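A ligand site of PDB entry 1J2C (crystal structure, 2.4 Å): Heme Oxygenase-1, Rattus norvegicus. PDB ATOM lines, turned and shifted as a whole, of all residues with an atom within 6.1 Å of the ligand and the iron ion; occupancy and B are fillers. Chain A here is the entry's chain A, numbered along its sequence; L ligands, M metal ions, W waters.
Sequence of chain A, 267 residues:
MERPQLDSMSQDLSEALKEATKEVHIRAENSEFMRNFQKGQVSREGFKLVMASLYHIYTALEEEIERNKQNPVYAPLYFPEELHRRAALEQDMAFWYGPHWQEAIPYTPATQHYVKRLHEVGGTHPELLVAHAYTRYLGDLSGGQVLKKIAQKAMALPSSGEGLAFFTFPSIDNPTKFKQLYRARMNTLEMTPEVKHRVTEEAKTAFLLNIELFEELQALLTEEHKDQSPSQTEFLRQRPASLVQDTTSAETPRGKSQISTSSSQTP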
ATOM      1  N   SER A  14     -36.630 -10.605  17.494  1.00  0.00           N
ATOM      2  CA  SER A  14     -36.165 -11.752  16.705  1.00  0.00           C
ATOM      3  C   SER A  14     -35.337 -11.306  15.509  1.00  0.00           C
ATOM      4  O   SER A  14     -34.373 -11.976  15.135  1.00  0.00           O
ATOM      5  CB  SER A  14     -37.349 -12.603  16.237  1.00  0.00           C
ATOM      6  OG  SER A  14     -38.222 -11.862  15.396  1.00  0.00           O
ATOM      7  N   LEU A  17     -31.946  -9.904  16.935  1.00  0.00           N
ATOM      8  CA  LEU A  17     -31.117 -11.024  17.359  1.00  0.00           C
ATOM      9  C   LEU A  17     -30.471 -11.744  16.187  1.00  0.00           C
ATOM     10  O   LEU A  17     -29.286 -12.087  16.233  1.00  0.00           O
ATOM     11  CB  LEU A  17     -31.948 -12.018  18.170  1.00  0.00           C
ATOM     12  CG  LEU A  17     -31.990 -11.754  19.674  1.00  0.00           C
ATOM     13  CD1 LEU A  17     -32.905 -12.766  20.354  1.00  0.00           C
ATOM     14  CD2 LEU A  17     -30.583 -11.862  20.235  1.00  0.00           C
ATOM     15  N   LYS A  18     -31.245 -11.978  15.135  1.00  0.00           N
ATOM     16  CA  LYS A  18     -30.718 -12.670  13.959  1.00  0.00           C
ATOM     17  C   LYS A  18     -29.621 -11.841  13.277  1.00  0.00           C
ATOM     18  O   LYS A  18     -28.563 -12.375  12.933  1.00  0.00           O
ATOM     19  CB  LYS A  18     -31.848 -12.947  12.969  1.00  0.00           C
ATOM     20  CG  LYS A  18     -31.423 -13.737  11.741  1.00  0.00           C
ATOM     21  CD  LYS A  18     -32.566 -13.868  10.753  1.00  0.00           C
ATOM     22  CE  LYS A  18     -32.115 -14.566   9.482  1.00  0.00           C
ATOM     23  NZ  LYS A  18     -31.519 -15.902   9.796  1.00  0.00           N
ATOM     24  N   THR A  21     -26.378 -11.716  15.618  1.00  0.00           N
ATOM     25  CA  THR A  21     -25.567 -12.910  15.781  1.00  0.00           C
ATOM     26  C   THR A  21     -25.135 -13.609  14.495  1.00  0.00           C
ATOM     27  O   THR A  21     -24.410 -14.608  14.555  1.00  0.00           O
ATOM     28  CB  THR A  21     -26.313 -13.939  16.660  1.00  0.00           C
ATOM     29  OG1 THR A  21     -27.507 -14.360  15.979  1.00  0.00           O
ATOM     30  CG2 THR A  21     -26.692 -13.327  18.000  1.00  0.00           C
ATOM     31  N   HIS A  25     -22.116 -16.258  14.367  1.00  0.00           N
ATOM     32  CA  HIS A  25     -22.687 -17.561  14.051  1.00  0.00           C
ATOM     33  C   HIS A  25     -21.836 -18.265  12.994  1.00  0.00           C
ATOM     34  O   HIS A  25     -21.563 -19.456  13.088  1.00  0.00           O
ATOM     35  CB  HIS A  25     -24.126 -17.437  13.536  1.00  0.00           C
ATOM     36  CG  HIS A  25     -24.744 -18.757  13.156  1.00  0.00           C
ATOM     37  ND1 HIS A  25     -24.417 -19.421  11.995  1.00  0.00           N
ATOM     38  CD2 HIS A  25     -25.608 -19.551  13.822  1.00  0.00           C
ATOM     39  CE1 HIS A  25     -25.058 -20.579  11.960  1.00  0.00           C
ATOM     40  NE2 HIS A  25     -25.785 -20.679  13.064  1.00  0.00           N
ATOM     41  N   ALA A  28     -18.875 -19.452  14.683  1.00  0.00           N
ATOM     42  CA  ALA A  28     -19.183 -20.597  15.531  1.00  0.00           C
ATOM     43  C   ALA A  28     -19.421 -21.851  14.691  1.00  0.00           C
ATOM     44  O   ALA A  28     -18.967 -22.945  15.028  1.00  0.00           O
ATOM     45  CB  ALA A  28     -20.411 -20.311  16.385  1.00  0.00           C
ATOM     46  N   GLU A  29     -20.113 -21.677  13.577  1.00  0.00           N
ATOM     47  CA  GLU A  29     -20.411 -22.774  12.671  1.00  0.00           C
ATOM     48  C   GLU A  29     -19.149 -23.361  12.037  1.00  0.00           C
ATOM     49  O   GLU A  29     -19.086 -24.562  11.763  1.00  0.00           O
ATOM     50  CB  GLU A  29     -21.362 -22.286  11.583  1.00  0.00           C
ATOM     51  CG  GLU A  29     -21.721 -23.345  10.552  1.00  0.00           C
ATOM     52  CD  GLU A  29     -22.524 -22.762   9.397  1.00  0.00           C
ATOM     53  OE1 GLU A  29     -22.804 -23.525   8.433  1.00  0.00           O
ATOM     54  OE2 GLU A  29     -22.875 -21.563   9.449  1.00  0.00           O
ATOM     55  N   MET A  34     -16.617 -28.141  15.381  1.00  0.00           N
ATOM     56  CA  MET A  34     -17.853 -28.258  14.616  1.00  0.00           C
ATOM     57  C   MET A  34     -17.540 -28.651  13.191  1.00  0.00           C
ATOM     58  O   MET A  34     -18.188 -29.520  12.622  1.00  0.00           O
ATOM     59  CB  MET A  34     -18.617 -26.939  14.605  1.00  0.00           C
ATOM     60  CG  MET A  34     -19.557 -26.788  15.770  1.00  0.00           C
ATOM     61  SD  MET A  34     -20.602 -28.252  15.913  1.00  0.00           S
ATOM     62  CE  MET A  34     -19.803 -29.049  17.321  1.00  0.00           C
ATOM     63  N   GLN A  38     -19.065 -31.738  11.332  1.00  0.00           N
ATOM     64  CA  GLN A  38     -19.788 -31.529  10.081  1.00  0.00           C
ATOM     65  C   GLN A  38     -19.306 -32.471   8.984  1.00  0.00           C
ATOM     66  O   GLN A  38     -20.119 -33.005   8.219  1.00  0.00           O
ATOM     67  CB  GLN A  38     -19.628 -30.090   9.598  1.00  0.00           C
ATOM     68  CG  GLN A  38     -20.922 -29.286   9.524  1.00  0.00           C
ATOM     69  CD  GLN A  38     -21.243 -28.570  10.820  1.00  0.00           C
ATOM     70  OE1 GLN A  38     -22.098 -27.671  10.850  1.00  0.00           O
ATOM     71  NE2 GLN A  38     -20.568 -28.943  11.903  1.00  0.00           N
ATOM     72  N   TYR A 114     -19.124 -21.091  31.125  1.00  0.00           N
ATOM     73  CA  TYR A 114     -20.437 -20.958  30.493  1.00  0.00           C
ATOM     74  C   TYR A 114     -21.505 -21.071  31.582  1.00  0.00           C
ATOM     75  O   TYR A 114     -22.396 -20.214  31.690  1.00  0.00           O
ATOM     76  CB  TYR A 114     -20.628 -22.076  29.458  1.00  0.00           C
ATOM     77  CG  TYR A 114     -21.671 -21.847  28.390  1.00  0.00           C
ATOM     78  CD1 TYR A 114     -22.824 -21.082  28.631  1.00  0.00           C
ATOM     79  CD2 TYR A 114     -21.548 -22.464  27.146  1.00  0.00           C
ATOM     80  CE1 TYR A 114     -23.817 -20.960  27.663  1.00  0.00           C
ATOM     81  CE2 TYR A 114     -22.532 -22.356  26.181  1.00  0.00           C
ATOM     82  CZ  TYR A 114     -23.667 -21.604  26.440  1.00  0.00           C
ATOM     83  OH  TYR A 114     -24.641 -21.510  25.478  1.00  0.00           O
ATOM     84  N   TYR A 134     -32.561 -18.624  23.437  1.00  0.00           N
ATOM     85  CA  TYR A 134     -32.582 -18.406  21.996  1.00  0.00           C
ATOM     86  C   TYR A 134     -31.380 -19.075  21.324  1.00  0.00           C
ATOM     87  O   TYR A 134     -31.524 -19.882  20.402  1.00  0.00           O
ATOM     88  CB  TYR A 134     -32.540 -16.898  21.711  1.00  0.00           C
ATOM     89  CG  TYR A 134     -32.105 -16.531  20.316  1.00  0.00           C
ATOM     90  CD1 TYR A 134     -32.981 -16.652  19.224  1.00  0.00           C
ATOM     91  CD2 TYR A 134     -30.817 -16.038  20.076  1.00  0.00           C
ATOM     92  CE1 TYR A 134     -32.582 -16.272  17.933  1.00  0.00           C
ATOM     93  CE2 TYR A 134     -30.408 -15.670  18.801  1.00  0.00           C
ATOM     94  CZ  TYR A 134     -31.296 -15.786  17.737  1.00  0.00           C
ATOM     95  OH  TYR A 134     -30.879 -15.408  16.482  1.00  0.00           O
ATOM     96  N   THR A 135     -30.200 -18.744  21.818  1.00  0.00           N
ATOM     97  CA  THR A 135     -28.949 -19.249  21.278  1.00  0.00           C
ATOM     98  C   THR A 135     -28.862 -20.773  21.220  1.00  0.00           C
ATOM     99  O   THR A 135     -28.548 -21.338  20.177  1.00  0.00           O
ATOM    100  CB  THR A 135     -27.765 -18.664  22.073  1.00  0.00           C
ATOM    101  OG1 THR A 135     -27.562 -17.302  21.663  1.00  0.00           O
ATOM    102  CG2 THR A 135     -26.484 -19.454  21.849  1.00  0.00           C
ATOM    103  N   ARG A 136     -29.135 -21.448  22.339  1.00  0.00           N
ATOM    104  CA  ARG A 136     -29.060 -22.907  22.362  1.00  0.00           C
ATOM    105  C   ARG A 136     -30.256 -23.614  21.689  1.00  0.00           C
ATOM    106  O   ARG A 136     -30.077 -24.384  20.748  1.00  0.00           O
ATOM    107  CB  ARG A 136     -28.942 -23.410  23.808  1.00  0.00           C
ATOM    108  CG  ARG A 136     -27.587 -23.177  24.493  1.00  0.00           C
ATOM    109  CD  ARG A 136     -26.382 -23.712  23.683  1.00  0.00           C
ATOM    110  NE  ARG A 136     -26.609 -25.041  23.122  1.00  0.00           N
ATOM    111  CZ  ARG A 136     -25.775 -25.637  22.261  1.00  0.00           C
ATOM    112  NH1 ARG A 136     -24.664 -25.033  21.863  1.00  0.00           N
ATOM    113  NH2 ARG A 136     -26.070 -26.837  21.761  1.00  0.00           N
ATOM    114  N   LEU A 138     -32.812 -22.619  19.593  1.00  0.00           N
ATOM    115  CA  LEU A 138     -33.025 -22.463  18.154  1.00  0.00           C
ATOM    116  C   LEU A 138     -31.929 -23.161  17.366  1.00  0.00           C
ATOM    117  O   LEU A 138     -32.195 -23.720  16.302  1.00  0.00           O
ATOM    118  CB  LEU A 138     -33.129 -20.979  17.765  1.00  0.00           C
ATOM    119  CG  LEU A 138     -34.383 -20.196  18.206  1.00  0.00           C
ATOM    120  CD1 LEU A 138     -34.883 -19.349  17.055  1.00  0.00           C
ATOM    121  CD2 LEU A 138     -35.502 -21.154  18.638  1.00  0.00           C
ATOM    122  N   GLY A 139     -30.703 -23.131  17.873  1.00  0.00           N
ATOM    123  CA  GLY A 139     -29.622 -23.810  17.197  1.00  0.00           C
ATOM    124  C   GLY A 139     -29.896 -25.305  17.152  1.00  0.00           C
ATOM    125  O   GLY A 139     -29.677 -25.968  16.129  1.00  0.00           O
ATOM    126  N   ASP A 140     -30.383 -25.854  18.267  1.00  0.00           N
ATOM    127  CA  ASP A 140     -30.689 -27.273  18.323  1.00  0.00           C
ATOM    128  C   ASP A 140     -31.759 -27.601  17.301  1.00  0.00           C
ATOM    129  O   ASP A 140     -31.655 -28.610  16.614  1.00  0.00           O
ATOM    130  CB  ASP A 140     -31.185 -27.673  19.714  1.00  0.00           C
ATOM    131  CG  ASP A 140     -30.151 -27.397  20.793  1.00  0.00           C
ATOM    132  OD1 ASP A 140     -28.940 -27.396  20.470  1.00  0.00           O
ATOM    133  OD2 ASP A 140     -30.569 -27.215  21.963  1.00  0.00           O
ATOM    134  N   SER A 142     -32.296 -26.152  14.598  1.00  0.00           N
ATOM    135  CA  SER A 142     -31.838 -25.887  13.243  1.00  0.00           C
ATOM    136  C   SER A 142     -30.823 -26.919  12.741  1.00  0.00           C
ATOM    137  O   SER A 142     -31.011 -27.523  11.688  1.00  0.00           O
ATOM    138  CB  SER A 142     -31.242 -24.486  13.176  1.00  0.00           C
ATOM    139  OG  SER A 142     -32.187 -23.532  13.617  1.00  0.00           O
ATOM    140  N   GLY A 143     -29.750 -27.112  13.495  1.00  0.00           N
ATOM    141  CA  GLY A 143     -28.747 -28.071  13.080  1.00  0.00           C
ATOM    142  C   GLY A 143     -28.905 -29.380  13.813  1.00  0.00           C
ATOM    143  O   GLY A 143     -28.085 -30.289  13.675  1.00  0.00           O
ATOM    144  N   GLY A 144     -29.966 -29.480  14.606  1.00  0.00           N
ATOM    145  CA  GLY A 144     -30.212 -30.678  15.373  1.00  0.00           C
ATOM    146  C   GLY A 144     -30.273 -31.957  14.568  1.00  0.00           C
ATOM    147  O   GLY A 144     -29.495 -32.882  14.819  1.00  0.00           O
ATOM    148  N   VAL A 146     -29.308 -32.429  11.650  1.00  0.00           N
ATOM    149  CA  VAL A 146     -28.116 -32.570  10.833  1.00  0.00           C
ATOM    150  C   VAL A 146     -26.997 -33.270  11.615  1.00  0.00           C
ATOM    151  O   VAL A 146     -26.476 -34.286  11.179  1.00  0.00           O
ATOM    152  CB  VAL A 146     -27.627 -31.203  10.329  1.00  0.00           C
ATOM    153  CG1 VAL A 146     -26.290 -31.339   9.627  1.00  0.00           C
ATOM    154  CG2 VAL A 146     -28.662 -30.630   9.380  1.00  0.00           C
ATOM    155  N   LEU A 147     -26.647 -32.720  12.778  1.00  0.00           N
ATOM    156  CA  LEU A 147     -25.596 -33.327  13.583  1.00  0.00           C
ATOM    157  C   LEU A 147     -26.000 -34.749  13.957  1.00  0.00           C
ATOM    158  O   LEU A 147     -25.161 -35.645  14.026  1.00  0.00           O
ATOM    159  CB  LEU A 147     -25.351 -32.509  14.852  1.00  0.00           C
ATOM    160  CG  LEU A 147     -24.866 -31.064  14.671  1.00  0.00           C
ATOM    161  CD1 LEU A 147     -24.635 -30.442  16.046  1.00  0.00           C
ATOM    162  CD2 LEU A 147     -23.576 -31.039  13.845  1.00  0.00           C
ATOM    163  N   LYS A 179     -40.086 -22.973  15.481  1.00  0.00           N
ATOM    164  CA  LYS A 179     -39.096 -21.901  15.462  1.00  0.00           C
ATOM    165  C   LYS A 179     -39.822 -20.598  15.125  1.00  0.00           C
ATOM    166  O   LYS A 179     -39.581 -19.555  15.744  1.00  0.00           O
ATOM    167  CB  LYS A 179     -38.028 -22.214  14.404  1.00  0.00           C
ATOM    168  CG  LYS A 179     -36.595 -22.243  14.924  1.00  0.00           C
ATOM    169  CD  LYS A 179     -35.779 -23.398  14.318  1.00  0.00           C
ATOM    170  CE  LYS A 179     -35.765 -23.429  12.779  1.00  0.00           C
ATOM    171  NZ  LYS A 179     -35.067 -22.259  12.154  1.00  0.00           N
ATOM    172  N   ARG A 183     -40.040 -17.411  17.565  1.00  0.00           N
ATOM    173  CA  ARG A 183     -39.589 -16.079  17.180  1.00  0.00           C
ATOM    174  C   ARG A 183     -40.690 -15.060  17.407  1.00  0.00           C
ATOM    175  O   ARG A 183     -40.441 -13.976  17.933  1.00  0.00           O
ATOM    176  CB  ARG A 183     -39.173 -16.025  15.710  1.00  0.00           C
ATOM    177  CG  ARG A 183     -37.945 -16.829  15.350  1.00  0.00           C
ATOM    178  CD  ARG A 183     -37.461 -16.464  13.958  1.00  0.00           C
ATOM    179  NE  ARG A 183     -36.371 -17.332  13.516  1.00  0.00           N
ATOM    180  CZ  ARG A 183     -36.553 -18.532  12.964  1.00  0.00           C
ATOM    181  NH1 ARG A 183     -37.787 -19.008  12.780  1.00  0.00           N
ATOM    182  NH2 ARG A 183     -35.503 -19.267  12.612  1.00  0.00           N
ATOM    183  N   ALA A 206     -23.178 -15.486  24.286  1.00  0.00           N
ATOM    184  CA  ALA A 206     -23.542 -16.898  24.316  1.00  0.00           C
ATOM    185  C   ALA A 206     -22.811 -17.640  23.209  1.00  0.00           C
ATOM    186  O   ALA A 206     -22.259 -18.718  23.419  1.00  0.00           O
ATOM    187  CB  ALA A 206     -25.054 -17.063  24.142  1.00  0.00           C
ATOM    188  N   PHE A 207     -22.819 -17.064  22.008  1.00  0.00           N
ATOM    189  CA  PHE A 207     -22.143 -17.698  20.887  1.00  0.00           C
ATOM    190  C   PHE A 207     -20.661 -17.843  21.171  1.00  0.00           C
ATOM    191  O   PHE A 207     -20.068 -18.874  20.878  1.00  0.00           O
ATOM    192  CB  PHE A 207     -22.337 -16.904  19.602  1.00  0.00           C
ATOM    193  CG  PHE A 207     -23.594 -17.262  18.850  1.00  0.00           C
ATOM    194  CD1 PHE A 207     -24.792 -16.593  19.105  1.00  0.00           C
ATOM    195  CD2 PHE A 207     -23.574 -18.263  17.891  1.00  0.00           C
ATOM    196  CE1 PHE A 207     -25.951 -16.938  18.420  1.00  0.00           C
ATOM    197  CE2 PHE A 207     -24.723 -18.616  17.201  1.00  0.00           C
ATOM    198  CZ  PHE A 207     -25.922 -17.945  17.470  1.00  0.00           C
ATOM    199  N   ASN A 210     -19.895 -20.579  23.444  1.00  0.00           N
ATOM    200  CA  ASN A 210     -19.982 -21.846  22.742  1.00  0.00           C
ATOM    201  C   ASN A 210     -18.714 -22.074  21.945  1.00  0.00           C
ATOM    202  O   ASN A 210     -18.207 -23.185  21.871  1.00  0.00           O
ATOM    203  CB  ASN A 210     -21.193 -21.843  21.807  1.00  0.00           C
ATOM    204  CG  ASN A 210     -22.472 -22.210  22.528  1.00  0.00           C
ATOM    205  OD1 ASN A 210     -22.756 -23.387  22.743  1.00  0.00           O
ATOM    206  ND2 ASN A 210     -23.242 -21.202  22.925  1.00  0.00           N
ATOM    207  N   PHE A 214     -15.843 -25.141  22.344  1.00  0.00           N
ATOM    208  CA  PHE A 214     -15.356 -25.964  21.233  1.00  0.00           C
ATOM    209  C   PHE A 214     -13.841 -25.913  21.081  1.00  0.00           C
ATOM    210  O   PHE A 214     -13.195 -26.949  20.899  1.00  0.00           O
ATOM    211  CB  PHE A 214     -16.026 -25.544  19.926  1.00  0.00           C
ATOM    212  CG  PHE A 214     -17.519 -25.774  19.916  1.00  0.00           C
ATOM    213  CD1 PHE A 214     -18.061 -26.967  20.416  1.00  0.00           C
ATOM    214  CD2 PHE A 214     -18.382 -24.809  19.417  1.00  0.00           C
ATOM    215  CE1 PHE A 214     -19.434 -27.178  20.430  1.00  0.00           C
ATOM    216  CE2 PHE A 214     -19.774 -25.006  19.427  1.00  0.00           C
ATOM    217  CZ  PHE A 214     -20.296 -26.196  19.943  1.00  0.00           C
HETATM  218  C1  LIG L   1     -30.008 -21.117  12.757  1.00  0.00           C
HETATM  219  N1  LIG L   1     -28.265 -22.556  11.837  1.00  0.00           N
HETATM  220  C2  LIG L   1     -29.428 -21.837  11.690  1.00  0.00           C
HETATM  221  C3  LIG L   1     -30.051 -22.160  10.380  1.00  0.00           C
HETATM  222  C4  LIG L   1     -29.430 -23.337   9.999  1.00  0.00           C
HETATM  223  C5  LIG L   1     -28.253 -23.507  10.876  1.00  0.00           C
HETATM  224  C6  LIG L   1     -29.964 -24.404   9.033  1.00  0.00           C
HETATM  225  C7  LIG L   1     -30.903 -21.218   9.497  1.00  0.00           C
HETATM  226  C8  LIG L   1     -27.274 -24.542  10.847  1.00  0.00           C
HETATM  227  N2  LIG L   1     -26.937 -24.778  13.234  1.00  0.00           N
HETATM  228  C9  LIG L   1     -26.568 -25.094  11.942  1.00  0.00           C
HETATM  229  C10 LIG L   1     -25.469 -26.126  11.925  1.00  0.00           C
HETATM  230  C11 LIG L   1     -25.110 -26.275  13.284  1.00  0.00           C
HETATM  231  C12 LIG L   1     -26.217 -25.642  14.025  1.00  0.00           C
HETATM  232  C13 LIG L   1     -25.147 -27.102  10.790  1.00  0.00           C
HETATM  233  O1  LIG L   1     -26.293 -25.581  15.261  1.00  0.00           O
HETATM  234  N3  LIG L   1     -25.844 -22.615  15.472  1.00  0.00           N
HETATM  235  C14 LIG L   1     -24.473 -22.824  15.517  1.00  0.00           C
HETATM  236  C15 LIG L   1     -24.011 -22.890  16.895  1.00  0.00           C
HETATM  237  C16 LIG L   1     -25.042 -22.346  17.641  1.00  0.00           C
HETATM  238  C17 LIG L   1     -26.181 -22.099  16.687  1.00  0.00           C
HETATM  239  C18 LIG L   1     -22.548 -23.293  17.303  1.00  0.00           C
HETATM  240  O2  LIG L   1     -23.820 -23.325  14.573  1.00  0.00           O
HETATM  241  C19 LIG L   1     -24.955 -22.244  19.043  1.00  0.00           C
HETATM  242  C20 LIG L   1     -24.432 -21.178  19.837  1.00  0.00           C
HETATM  243  C21 LIG L   1     -27.297 -21.278  16.848  1.00  0.00           C
HETATM  244  N4  LIG L   1     -28.523 -21.552  14.724  1.00  0.00           N
HETATM  245  C22 LIG L   1     -28.260 -20.894  15.908  1.00  0.00           C
HETATM  246  C23 LIG L   1     -29.335 -19.952  16.157  1.00  0.00           C
HETATM  247  C24 LIG L   1     -30.103 -19.935  15.024  1.00  0.00           C
HETATM  248  C25 LIG L   1     -29.465 -20.798  14.057  1.00  0.00           C
HETATM  249  C26 LIG L   1     -29.650 -19.251  17.492  1.00  0.00           C
HETATM  250  C27 LIG L   1     -31.173 -18.915  14.693  1.00  0.00           C
HETATM  251  C28 LIG L   1     -30.915 -17.559  14.013  1.00  0.00           C
HETATM  252  C29 LIG L   1     -32.236 -16.906  13.770  1.00  0.00           C
HETATM  253  O3  LIG L   1     -33.069 -17.431  13.010  1.00  0.00           O
HETATM  254  O4  LIG L   1     -32.749 -16.026  14.661  1.00  0.00           O
HETATM  255 FE    FE M   1     -27.111 -22.609  13.749  1.00  0.00          FE
HETATM  256  O   HOH W   1     -25.762 -25.839  17.747  1.00  0.00           O
HETATM  257  O   HOH W   2     -27.313 -24.747  19.629  1.00  0.00           O
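Water W2 lies within hydrogen-bond range of the backbone carbonyl oxygen (O) of Arg 136 (3.0 Å) and the side-chain carboxylate (OD1) of Asp 140 (3.2 Å).
The side-chain hydroxyl (OH) of Tyr 134 is in hydrogen-bond range of an oxygen (O4) of the ligand (2.7 Å).
The side-chain amino group (NZ) of Lys 18 lies within salt-bridge range of an oxygen (O3) of the ligand.
The guanidinium group (NH2) of Arg 183 is in salt-bridge range of an oxygen (O3) of the ligand, at 3.1 Å.
The backbone carbonyl oxygen (O) of Leu 138 is in hydrogen-bond range of the side-chain hydroxyl (OG) of Ser 142 (2.7 Å).
The guanidinium group (NH1) of Arg 136 sits at hydrogen-bond distance from the side-chain amide oxygen (OD1) of Asn 210, 2.7 Å away.
The side-chain hydroxyl (OG) of Ser 142 is in hydrogen-bond range of the side-chain amino group (NZ) of Lys 179 (3.5 Å).
The backbone carbonyl oxygen (O) of Ala 206 lies within hydrogen-bond range of the side-chain amide nitrogen (ND2) of Asn 210, at 2.7 Å.
The backbone carbonyl oxygen of Met 34 lies within hydrogen-bond range of the side-chain amide nitrogen of Gln 38 (2.6 Å).
ND2 of Asn 210 sits at hydrogen-bond distance from OH of Tyr 114.
The guanidinium group (NH2) of Arg 136 is in salt-bridge range of the side-chain carboxylate (OD1) of Asp 140, at 3.2 Å.
The iron ion is bound by a nitrogen (N4) of the ligand (2.0 Å), a nitrogen (N3) of the ligand (2.1 Å), a nitrogen (N1) of the ligand (2.2 Å), a nitrogen (N2) of the ligand (2.2 Å) and a ring nitrogen (NE2) of His 25 (2.4 Å).
CB of Ala 28 touches C18 of the ligand, 3.8 Å away.
Glu 29 touches the ligand (CA to O2, 3.9 Å).
Gln 38 touches the ligand.
Thr 135 touches the ligand.
NH1 of Arg 136 touches C19 of the ligand, at 3.98 Å.
Leu 138 touches the ligand.
Gly 139 touches the ligand.
OG of Ser 142 touches C1 of the ligand (3.4 Å).
Gly 143 touches the ligand.
Phe 207 touches the ligand.
ND2 of Asn 210 touches C20 of the ligand, at 3.3 Å.
CE2 of Phe 214 touches C18 of the ligand (3.9 Å).
16 residues have an atom within 4 Å of the ligand: Lys 18, His 25, Ala 28, Glu 29, Gln 38, Tyr 134, Thr 135, Arg 136, Leu 138, Gly 139, Ser 142, Gly 143, Arg 183, Phe 207, Asn 210 and Phe 214.
Of the 27 residues printed, 1 comes within 4 Å of the iron ion.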
